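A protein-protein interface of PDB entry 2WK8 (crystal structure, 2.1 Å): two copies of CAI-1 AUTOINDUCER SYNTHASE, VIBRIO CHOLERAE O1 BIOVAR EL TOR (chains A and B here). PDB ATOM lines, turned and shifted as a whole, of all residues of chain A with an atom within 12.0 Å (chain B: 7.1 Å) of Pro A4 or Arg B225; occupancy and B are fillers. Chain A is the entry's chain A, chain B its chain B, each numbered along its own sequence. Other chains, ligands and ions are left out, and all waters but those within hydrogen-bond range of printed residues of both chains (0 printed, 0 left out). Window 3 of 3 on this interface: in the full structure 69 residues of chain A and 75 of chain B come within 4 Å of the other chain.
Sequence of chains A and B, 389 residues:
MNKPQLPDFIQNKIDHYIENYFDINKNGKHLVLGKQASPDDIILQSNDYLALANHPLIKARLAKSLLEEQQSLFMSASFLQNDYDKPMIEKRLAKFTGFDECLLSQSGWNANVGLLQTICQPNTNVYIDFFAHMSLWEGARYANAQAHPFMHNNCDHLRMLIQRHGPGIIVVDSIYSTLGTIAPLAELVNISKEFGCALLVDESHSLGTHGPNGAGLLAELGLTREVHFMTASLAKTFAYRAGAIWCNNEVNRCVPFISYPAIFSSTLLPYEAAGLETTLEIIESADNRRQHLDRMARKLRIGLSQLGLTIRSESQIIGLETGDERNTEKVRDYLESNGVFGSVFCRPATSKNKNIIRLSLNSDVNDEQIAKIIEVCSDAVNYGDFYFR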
ATOM      1  N   PRO A   4     -24.958  -4.166  -4.798  1.00  0.00           N
ATOM      2  CA  PRO A   4     -24.537  -5.100  -3.745  1.00  0.00           C
ATOM      3  C   PRO A   4     -25.460  -5.001  -2.543  1.00  0.00           C
ATOM      4  O   PRO A   4     -26.556  -4.452  -2.664  1.00  0.00           O
ATOM      5  CB  PRO A   4     -23.137  -4.612  -3.375  1.00  0.00           C
ATOM      6  CG  PRO A   4     -22.649  -3.933  -4.592  1.00  0.00           C
ATOM      7  CD  PRO A   4     -23.855  -3.303  -5.246  1.00  0.00           C
ATOM      8  N   GLN A   5     -25.032  -5.526  -1.401  1.00  0.00           N
ATOM      9  CA  GLN A   5     -25.871  -5.512  -0.210  1.00  0.00           C
ATOM     10  C   GLN A   5     -25.057  -5.069   0.978  1.00  0.00           C
ATOM     11  O   GLN A   5     -24.109  -5.754   1.377  1.00  0.00           O
ATOM     12  CB  GLN A   5     -26.472  -6.889   0.041  1.00  0.00           C
ATOM     13  N   LEU A   6     -25.424  -3.923   1.540  1.00  0.00           N
ATOM     14  CA  LEU A   6     -24.692  -3.358   2.662  1.00  0.00           C
ATOM     15  C   LEU A   6     -24.871  -4.180   3.922  1.00  0.00           C
ATOM     16  O   LEU A   6     -25.986  -4.541   4.288  1.00  0.00           O
ATOM     17  CB  LEU A   6     -25.122  -1.913   2.928  1.00  0.00           C
ATOM     18  CG  LEU A   6     -24.465  -0.831   2.072  1.00  0.00           C
ATOM     19  CD1 LEU A   6     -25.174   0.495   2.285  1.00  0.00           C
ATOM     20  CD2 LEU A   6     -22.977  -0.719   2.391  1.00  0.00           C
ATOM     21  N   PRO A   7     -23.759  -4.457   4.601  1.00  0.00           N
ATOM     22  CA  PRO A   7     -23.782  -5.129   5.900  1.00  0.00           C
ATOM     23  C   PRO A   7     -24.742  -4.414   6.837  1.00  0.00           C
ATOM     24  O   PRO A   7     -24.892  -3.193   6.722  1.00  0.00           O
ATOM     25  CB  PRO A   7     -22.355  -4.951   6.398  1.00  0.00           C
ATOM     26  CG  PRO A   7     -21.528  -4.782   5.144  1.00  0.00           C
ATOM     27  CD  PRO A   7     -22.406  -4.037   4.199  1.00  0.00           C
ATOM     28  N   ASP A   8     -25.382  -5.154   7.740  1.00  0.00           N
ATOM     29  CA  ASP A   8     -26.307  -4.556   8.701  1.00  0.00           C
ATOM     30  C   ASP A   8     -25.657  -3.410   9.469  1.00  0.00           C
ATOM     31  O   ASP A   8     -26.314  -2.409   9.761  1.00  0.00           O
ATOM     32  CB  ASP A   8     -26.809  -5.598   9.705  1.00  0.00           C
ATOM     33  CG  ASP A   8     -27.719  -6.639   9.077  1.00  0.00           C
ATOM     34  OD1 ASP A   8     -28.354  -6.348   8.034  1.00  0.00           O
ATOM     35  OD2 ASP A   8     -27.796  -7.754   9.642  1.00  0.00           O
ATOM     36  N   ILE A  10     -23.963  -1.146   8.625  1.00  0.00           N
ATOM     37  CA  ILE A  10     -23.979   0.104   7.888  1.00  0.00           C
ATOM     38  C   ILE A  10     -25.404   0.511   7.480  1.00  0.00           C
ATOM     39  O   ILE A  10     -25.795   1.673   7.625  1.00  0.00           O
ATOM     40  CB  ILE A  10     -23.060   0.035   6.641  1.00  0.00           C
ATOM     41  CG1 ILE A  10     -21.612  -0.209   7.066  1.00  0.00           C
ATOM     42  CG2 ILE A  10     -23.163   1.317   5.823  1.00  0.00           C
ATOM     43  CD1 ILE A  10     -20.647  -0.292   5.896  1.00  0.00           C
ATOM     44  N   GLN A  11     -26.174  -0.434   6.954  1.00  0.00           N
ATOM     45  CA  GLN A  11     -27.486  -0.095   6.434  1.00  0.00           C
ATOM     46  C   GLN A  11     -28.269   0.564   7.537  1.00  0.00           C
ATOM     47  O   GLN A  11     -28.986   1.546   7.324  1.00  0.00           O
ATOM     48  CB  GLN A  11     -28.243  -1.331   5.973  1.00  0.00           C
ATOM     49  CG  GLN A  11     -29.530  -0.984   5.245  1.00  0.00           C
ATOM     50  CD  GLN A  11     -29.272  -0.335   3.899  1.00  0.00           C
ATOM     51  OE1 GLN A  11     -29.707   0.788   3.644  1.00  0.00           O
ATOM     52  NE2 GLN A  11     -28.551  -1.037   3.028  1.00  0.00           N
ATOM     53  N   ILE A  14     -27.299   4.117   8.168  1.00  0.00           N
ATOM     54  CA  ILE A  14     -27.859   4.950   7.109  1.00  0.00           C
ATOM     55  C   ILE A  14     -29.359   5.159   7.302  1.00  0.00           C
ATOM     56  O   ILE A  14     -29.849   6.289   7.266  1.00  0.00           O
ATOM     57  CB  ILE A  14     -27.591   4.361   5.715  1.00  0.00           C
ATOM     58  CG1 ILE A  14     -26.087   4.351   5.434  1.00  0.00           C
ATOM     59  CG2 ILE A  14     -28.329   5.163   4.643  1.00  0.00           C
ATOM     60  CD1 ILE A  14     -25.367   5.570   5.976  1.00  0.00           C
ATOM     61  N   ASP A  15     -30.075   4.059   7.504  1.00  0.00           N
ATOM     62  CA  ASP A  15     -31.508   4.097   7.752  1.00  0.00           C
ATOM     63  C   ASP A  15     -31.869   4.983   8.939  1.00  0.00           C
ATOM     64  O   ASP A  15     -32.771   5.804   8.850  1.00  0.00           O
ATOM     65  CB  ASP A  15     -32.025   2.683   7.989  1.00  0.00           C
ATOM     66  CG  ASP A  15     -31.955   1.830   6.746  1.00  0.00           C
ATOM     67  OD1 ASP A  15     -31.708   2.392   5.657  1.00  0.00           O
ATOM     68  OD2 ASP A  15     -32.145   0.605   6.854  1.00  0.00           O
ATOM     69  N   ALA B  94     -20.447   9.078 -12.272  1.00  0.00           N
ATOM     70  CA  ALA B  94     -21.127   7.867 -11.840  1.00  0.00           C
ATOM     71  C   ALA B  94     -21.381   6.962 -13.047  1.00  0.00           C
ATOM     72  O   ALA B  94     -21.064   5.777 -13.027  1.00  0.00           O
ATOM     73  CB  ALA B  94     -22.436   8.210 -11.119  1.00  0.00           C
ATOM     74  N   GLY B  98     -19.604   3.331 -13.630  1.00  0.00           N
ATOM     75  CA  GLY B  98     -20.584   2.280 -13.444  1.00  0.00           C
ATOM     76  C   GLY B  98     -21.229   2.208 -12.072  1.00  0.00           C
ATOM     77  O   GLY B  98     -22.079   1.348 -11.850  1.00  0.00           O
ATOM     78  N   PHE B  99     -20.843   3.095 -11.156  1.00  0.00           N
ATOM     79  CA  PHE B  99     -21.452   3.138  -9.818  1.00  0.00           C
ATOM     80  C   PHE B  99     -22.748   3.931  -9.820  1.00  0.00           C
ATOM     81  O   PHE B  99     -22.934   4.813 -10.660  1.00  0.00           O
ATOM     82  CB  PHE B  99     -20.483   3.734  -8.792  1.00  0.00           C
ATOM     83  CG  PHE B  99     -19.509   2.735  -8.232  1.00  0.00           C
ATOM     84  CD1 PHE B  99     -18.447   2.274  -8.998  1.00  0.00           C
ATOM     85  CD2 PHE B  99     -19.661   2.245  -6.945  1.00  0.00           C
ATOM     86  CE1 PHE B  99     -17.552   1.325  -8.494  1.00  0.00           C
ATOM     87  CE2 PHE B  99     -18.752   1.304  -6.421  1.00  0.00           C
ATOM     88  CZ  PHE B  99     -17.708   0.842  -7.204  1.00  0.00           C
ATOM     89  N   ASP B 100     -23.618   3.645  -8.854  1.00  0.00           N
ATOM     90  CA  ASP B 100     -24.939   4.281  -8.767  1.00  0.00           C
ATOM     91  C   ASP B 100     -24.877   5.790  -8.559  1.00  0.00           C
ATOM     92  O   ASP B 100     -25.730   6.520  -9.074  1.00  0.00           O
ATOM     93  CB  ASP B 100     -25.773   3.699  -7.611  1.00  0.00           C
ATOM     94  CG  ASP B 100     -26.267   2.288  -7.874  1.00  0.00           C
ATOM     95  OD1 ASP B 100     -26.184   1.795  -9.013  1.00  0.00           O
ATOM     96  OD2 ASP B 100     -26.757   1.663  -6.911  1.00  0.00           O
ATOM     97  N   GLU B 101     -23.894   6.252  -7.780  1.00  0.00           N
ATOM     98  CA  GLU B 101     -23.851   7.643  -7.354  1.00  0.00           C
ATOM     99  C   GLU B 101     -22.442   8.152  -7.211  1.00  0.00           C
ATOM    100  O   GLU B 101     -21.514   7.395  -6.894  1.00  0.00           O
ATOM    101  CB  GLU B 101     -24.565   7.815  -6.013  1.00  0.00           C
ATOM    102  CG  GLU B 101     -26.020   7.426  -6.058  1.00  0.00           C
ATOM    103  CD  GLU B 101     -26.813   8.330  -6.982  1.00  0.00           C
ATOM    104  OE1 GLU B 101     -26.256   9.368  -7.417  1.00  0.00           O
ATOM    105  OE2 GLU B 101     -27.991   8.007  -7.278  1.00  0.00           O
ATOM    106  N   LYS B 193     -18.043 -10.975   0.207  1.00  0.00           N
ATOM    107  CA  LYS B 193     -19.315 -11.690   0.086  1.00  0.00           C
ATOM    108  C   LYS B 193     -19.383 -12.811   1.113  1.00  0.00           C
ATOM    109  O   LYS B 193     -20.368 -12.939   1.839  1.00  0.00           O
ATOM    110  CB  LYS B 193     -19.462 -12.296  -1.311  1.00  0.00           C
ATOM    111  CG  LYS B 193     -20.056 -11.382  -2.363  1.00  0.00           C
ATOM    112  CD  LYS B 193     -20.226 -12.150  -3.677  1.00  0.00           C
ATOM    113  CE  LYS B 193     -20.719 -11.254  -4.809  1.00  0.00           C
ATOM    114  NZ  LYS B 193     -19.602 -10.517  -5.483  1.00  0.00           N
ATOM    115  N   LEU B 218     -11.725  -1.850 -11.399  1.00  0.00           N
ATOM    116  CA  LEU B 218     -12.991  -2.502 -11.089  1.00  0.00           C
ATOM    117  C   LEU B 218     -13.744  -2.734 -12.383  1.00  0.00           C
ATOM    118  O   LEU B 218     -14.197  -3.849 -12.647  1.00  0.00           O
ATOM    119  CB  LEU B 218     -13.820  -1.680 -10.119  1.00  0.00           C
ATOM    120  CG  LEU B 218     -13.261  -1.708  -8.700  1.00  0.00           C
ATOM    121  CD1 LEU B 218     -14.126  -0.859  -7.773  1.00  0.00           C
ATOM    122  CD2 LEU B 218     -13.154  -3.152  -8.212  1.00  0.00           C
ATOM    123  N   GLY B 222     -14.775  -6.328 -14.371  1.00  0.00           N
ATOM    124  CA  GLY B 222     -16.190  -6.638 -14.297  1.00  0.00           C
ATOM    125  C   GLY B 222     -16.694  -6.775 -12.871  1.00  0.00           C
ATOM    126  O   GLY B 222     -17.613  -7.543 -12.615  1.00  0.00           O
ATOM    127  N   LEU B 223     -16.100  -6.030 -11.941  1.00  0.00           N
ATOM    128  CA  LEU B 223     -16.437  -6.164 -10.529  1.00  0.00           C
ATOM    129  C   LEU B 223     -17.255  -4.988  -9.970  1.00  0.00           C
ATOM    130  O   LEU B 223     -17.647  -4.998  -8.807  1.00  0.00           O
ATOM    131  CB  LEU B 223     -15.159  -6.318  -9.700  1.00  0.00           C
ATOM    132  CG  LEU B 223     -14.325  -7.583  -9.910  1.00  0.00           C
ATOM    133  CD1 LEU B 223     -13.056  -7.514  -9.064  1.00  0.00           C
ATOM    134  CD2 LEU B 223     -15.149  -8.824  -9.593  1.00  0.00           C
ATOM    135  N   THR B 224     -17.489  -3.974 -10.795  1.00  0.00           N
ATOM    136  CA  THR B 224     -18.137  -2.748 -10.337  1.00  0.00           C
ATOM    137  C   THR B 224     -19.375  -3.004  -9.484  1.00  0.00           C
ATOM    138  O   THR B 224     -19.565  -2.382  -8.444  1.00  0.00           O
ATOM    139  CB  THR B 224     -18.570  -1.881 -11.522  1.00  0.00           C
ATOM    140  OG1 THR B 224     -17.453  -1.674 -12.397  1.00  0.00           O
ATOM    141  CG2 THR B 224     -19.108  -0.539 -11.015  1.00  0.00           C
ATOM    142  N   ARG B 225     -20.195  -3.947  -9.934  1.00  0.00           N
ATOM    143  CA  ARG B 225     -21.504  -4.196  -9.354  1.00  0.00           C
ATOM    144  C   ARG B 225     -21.498  -5.016  -8.080  1.00  0.00           C
ATOM    145  O   ARG B 225     -22.552  -5.275  -7.510  1.00  0.00           O
ATOM    146  CB  ARG B 225     -22.420  -4.843 -10.394  1.00  0.00           C
ATOM    147  CG  ARG B 225     -23.077  -3.805 -11.227  1.00  0.00           C
ATOM    148  CD  ARG B 225     -23.726  -2.849 -10.269  1.00  0.00           C
ATOM    149  NE  ARG B 225     -23.829  -1.481 -10.753  1.00  0.00           N
ATOM    150  CZ  ARG B 225     -24.508  -0.542 -10.101  1.00  0.00           C
ATOM    151  NH1 ARG B 225     -25.120  -0.862  -8.963  1.00  0.00           N
ATOM    152  NH2 ARG B 225     -24.582   0.701 -10.578  1.00  0.00           N
ATOM    153  N   GLU B 226     -20.321  -5.419  -7.627  1.00  0.00           N
ATOM    154  CA  GLU B 226     -20.225  -6.072  -6.327  1.00  0.00           C
ATOM    155  C   GLU B 226     -19.288  -5.383  -5.339  1.00  0.00           C
ATOM    156  O   GLU B 226     -18.918  -5.969  -4.321  1.00  0.00           O
ATOM    157  CB  GLU B 226     -19.858  -7.550  -6.476  1.00  0.00           C
ATOM    158  CG  GLU B 226     -19.005  -7.878  -7.676  1.00  0.00           C
ATOM    159  CD  GLU B 226     -19.457  -9.163  -8.338  1.00  0.00           C
ATOM    160  OE1 GLU B 226     -20.531  -9.660  -7.939  1.00  0.00           O
ATOM    161  OE2 GLU B 226     -18.757  -9.671  -9.250  1.00  0.00           O
ATOM    162  N   VAL B 227     -18.898  -4.150  -5.639  1.00  0.00           N
ATOM    163  CA  VAL B 227     -18.192  -3.328  -4.662  1.00  0.00           C
ATOM    164  C   VAL B 227     -19.142  -2.266  -4.117  1.00  0.00           C
ATOM    165  O   VAL B 227     -19.903  -1.651  -4.868  1.00  0.00           O
ATOM    166  CB  VAL B 227     -16.926  -2.665  -5.263  1.00  0.00           C
ATOM    167  CG1 VAL B 227     -16.304  -1.732  -4.274  1.00  0.00           C
ATOM    168  CG2 VAL B 227     -15.932  -3.729  -5.692  1.00  0.00           C
ATOM    169  N   HIS B 228     -19.111  -2.066  -2.808  1.00  0.00           N
ATOM    170  CA  HIS B 228     -19.991  -1.106  -2.171  1.00  0.00           C
ATOM    171  C   HIS B 228     -19.566   0.315  -2.450  1.00  0.00           C
ATOM    172  O   HIS B 228     -20.407   1.188  -2.695  1.00  0.00           O
ATOM    173  CB  HIS B 228     -20.037  -1.375  -0.670  1.00  0.00           C
ATOM    174  CG  HIS B 228     -20.482  -2.765  -0.339  1.00  0.00           C
ATOM    175  ND1 HIS B 228     -19.633  -3.853  -0.400  1.00  0.00           N
ATOM    176  CD2 HIS B 228     -21.696  -3.255   0.012  1.00  0.00           C
ATOM    177  CE1 HIS B 228     -20.300  -4.947  -0.075  1.00  0.00           C
ATOM    178  NE2 HIS B 228     -21.554  -4.612   0.181  1.00  0.00           N
ATOM    179  N   PHE B 229     -18.257   0.544  -2.415  1.00  0.00           N
ATOM    180  CA  PHE B 229     -17.726   1.899  -2.496  1.00  0.00           C
ATOM    181  C   PHE B 229     -16.437   1.941  -3.269  1.00  0.00           C
ATOM    182  O   PHE B 229     -15.604   1.043  -3.148  1.00  0.00           O
ATOM    183  CB  PHE B 229     -17.406   2.433  -1.106  1.00  0.00           C
ATOM    184  CG  PHE B 229     -18.530   2.344  -0.148  1.00  0.00           C
ATOM    185  CD1 PHE B 229     -18.558   1.346   0.814  1.00  0.00           C
ATOM    186  CD2 PHE B 229     -19.558   3.276  -0.182  1.00  0.00           C
ATOM    187  CE1 PHE B 229     -19.614   1.277   1.724  1.00  0.00           C
ATOM    188  CE2 PHE B 229     -20.596   3.210   0.712  1.00  0.00           C
ATOM    189  CZ  PHE B 229     -20.630   2.208   1.667  1.00  0.00           C
ATOM    190  N   CYS B 247     -20.745   5.400  -4.817  1.00  0.00           N
ATOM    191  CA  CYS B 247     -21.541   4.516  -3.971  1.00  0.00           C
ATOM    192  C   CYS B 247     -22.508   3.694  -4.789  1.00  0.00           C
ATOM    193  O   CYS B 247     -23.148   4.211  -5.703  1.00  0.00           O
ATOM    194  CB  CYS B 247     -22.333   5.326  -2.942  1.00  0.00           C
ATOM    195  SG  CYS B 247     -21.310   6.008  -1.625  1.00  0.00           S
ATOM    196  N   ASN B 248     -22.601   2.411  -4.459  1.00  0.00           N
ATOM    197  CA  ASN B 248     -23.590   1.533  -5.069  1.00  0.00           C
ATOM    198  C   ASN B 248     -24.728   1.328  -4.092  1.00  0.00           C
ATOM    199  O   ASN B 248     -25.227   0.216  -3.920  1.00  0.00           O
ATOM    200  CB  ASN B 248     -22.971   0.194  -5.461  1.00  0.00           C
ATOM    201  CG  ASN B 248     -22.346   0.227  -6.832  1.00  0.00           C
ATOM    202  OD1 ASN B 248     -22.797   0.956  -7.710  1.00  0.00           O
ATOM    203  ND2 ASN B 248     -21.302  -0.564  -7.029  1.00  0.00           N
ATOM    204  N   ASN B 249     -25.123   2.429  -3.460  1.00  0.00           N
ATOM    205  CA  ASN B 249     -26.103   2.438  -2.381  1.00  0.00           C
ATOM    206  C   ASN B 249     -26.427   3.895  -2.036  1.00  0.00           C
ATOM    207  O   ASN B 249     -26.175   4.788  -2.834  1.00  0.00           O
ATOM    208  CB  ASN B 249     -25.551   1.700  -1.164  1.00  0.00           C
ATOM    209  CG  ASN B 249     -24.149   2.160  -0.808  1.00  0.00           C
ATOM    210  OD1 ASN B 249     -23.953   3.318  -0.456  1.00  0.00           O
ATOM    211  ND2 ASN B 249     -23.160   1.259  -0.927  1.00  0.00           N
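The backbone carbonyl oxygen (O) of Gln A5 sits at hydrogen-bond distance from a ring nitrogen (NE2) of His B228, at 3.0 Å.
OD1 of Asp B100 is in salt-bridge range of NH2 of Arg B225, 2.5 Å away. The backbone NH of Asp B100 lies within hydrogen-bond range of the side-chain amide oxygen of Asn B248, 3.0 Å away. The side-chain amino group (NZ) of Lys B193 is in salt-bridge range of the side-chain carboxylate (OE1) of Glu B226 (2.8 Å). The backbone carbonyl oxygen (O) of Thr B224 lies within hydrogen-bond range of the side-chain amide nitrogen (ND2) of Asn B248, 2.9 Å away. OD1 of Asn B248 is in hydrogen-bond range of NH1 of Arg B225, 3.2 Å away. The side-chain amide nitrogen (ND2) of Asn B248 sits at hydrogen-bond distance from the backbone carbonyl oxygen (O) of Val B227, 2.8 Å away.
CG of Pro A4 touches O of Arg B225, at 3.2 Å. Glu B226 touches Pro A4. Pro A4 touches Val B227 (CG to O, 3.6 Å). Pro A4 touches His B228 (CB to NE2, 3.9 Å). Pro A4 touches Asn B248. CD2 of His B228 touches CD2 of Leu A6 (3.7 Å). CD2 of Leu A6 touches CZ of Phe B229, 3.8 Å away. Leu A6 touches Asn B249.
Printed residues of chain B within 4 Å of Pro A4: Arg B225, Glu B226, Val B227, His B228 and Asn B248. Arg B225 touches just one residue of chain A: Pro A4 (3.2 Å). No residue of chain A comes within 4 Å of Gly B98. No residue of chain A comes within 4 Å of Asp B100. No residue of chain A comes within 4 Å of Thr B224. Of chain A, only Pro A4 (3.7 Å) comes within 4 Å of Glu B226. Val B227 touches just one residue of chain A: Pro A4. Asn B248 touches just one residue of chain A: Pro A4. Of the printed residues of chain B, Gln A5 touches His B228. Of the printed residues of chain B, Leu A6 touches His B228, Phe B229 and Asn B249. Gln A11 touches none of the printed residues of chain B. The nearest residue of chain B that does not touch Pro A4 is Thr B224 (5.2 Å).
Of the 18 printed residues of chain B, 7 touch a printed residue of chain A. Hydrophobic or aromatic side chains of chain B that line the printed part of chain A: His B228 and Phe B229. Printed residues of chain A that touch a printed residue of chain B: Pro A4, Gln A5 and Leu A6. Along chain A the printed residues that touch a printed residue of chain B span positions 4 to 6. Among the printed residues, 9 pairs touch across the chains.
No position is printed for both chains. Of the 9 pairs that touch across the chains among the printed residues, none has its exchanged pair printed and touching as well.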
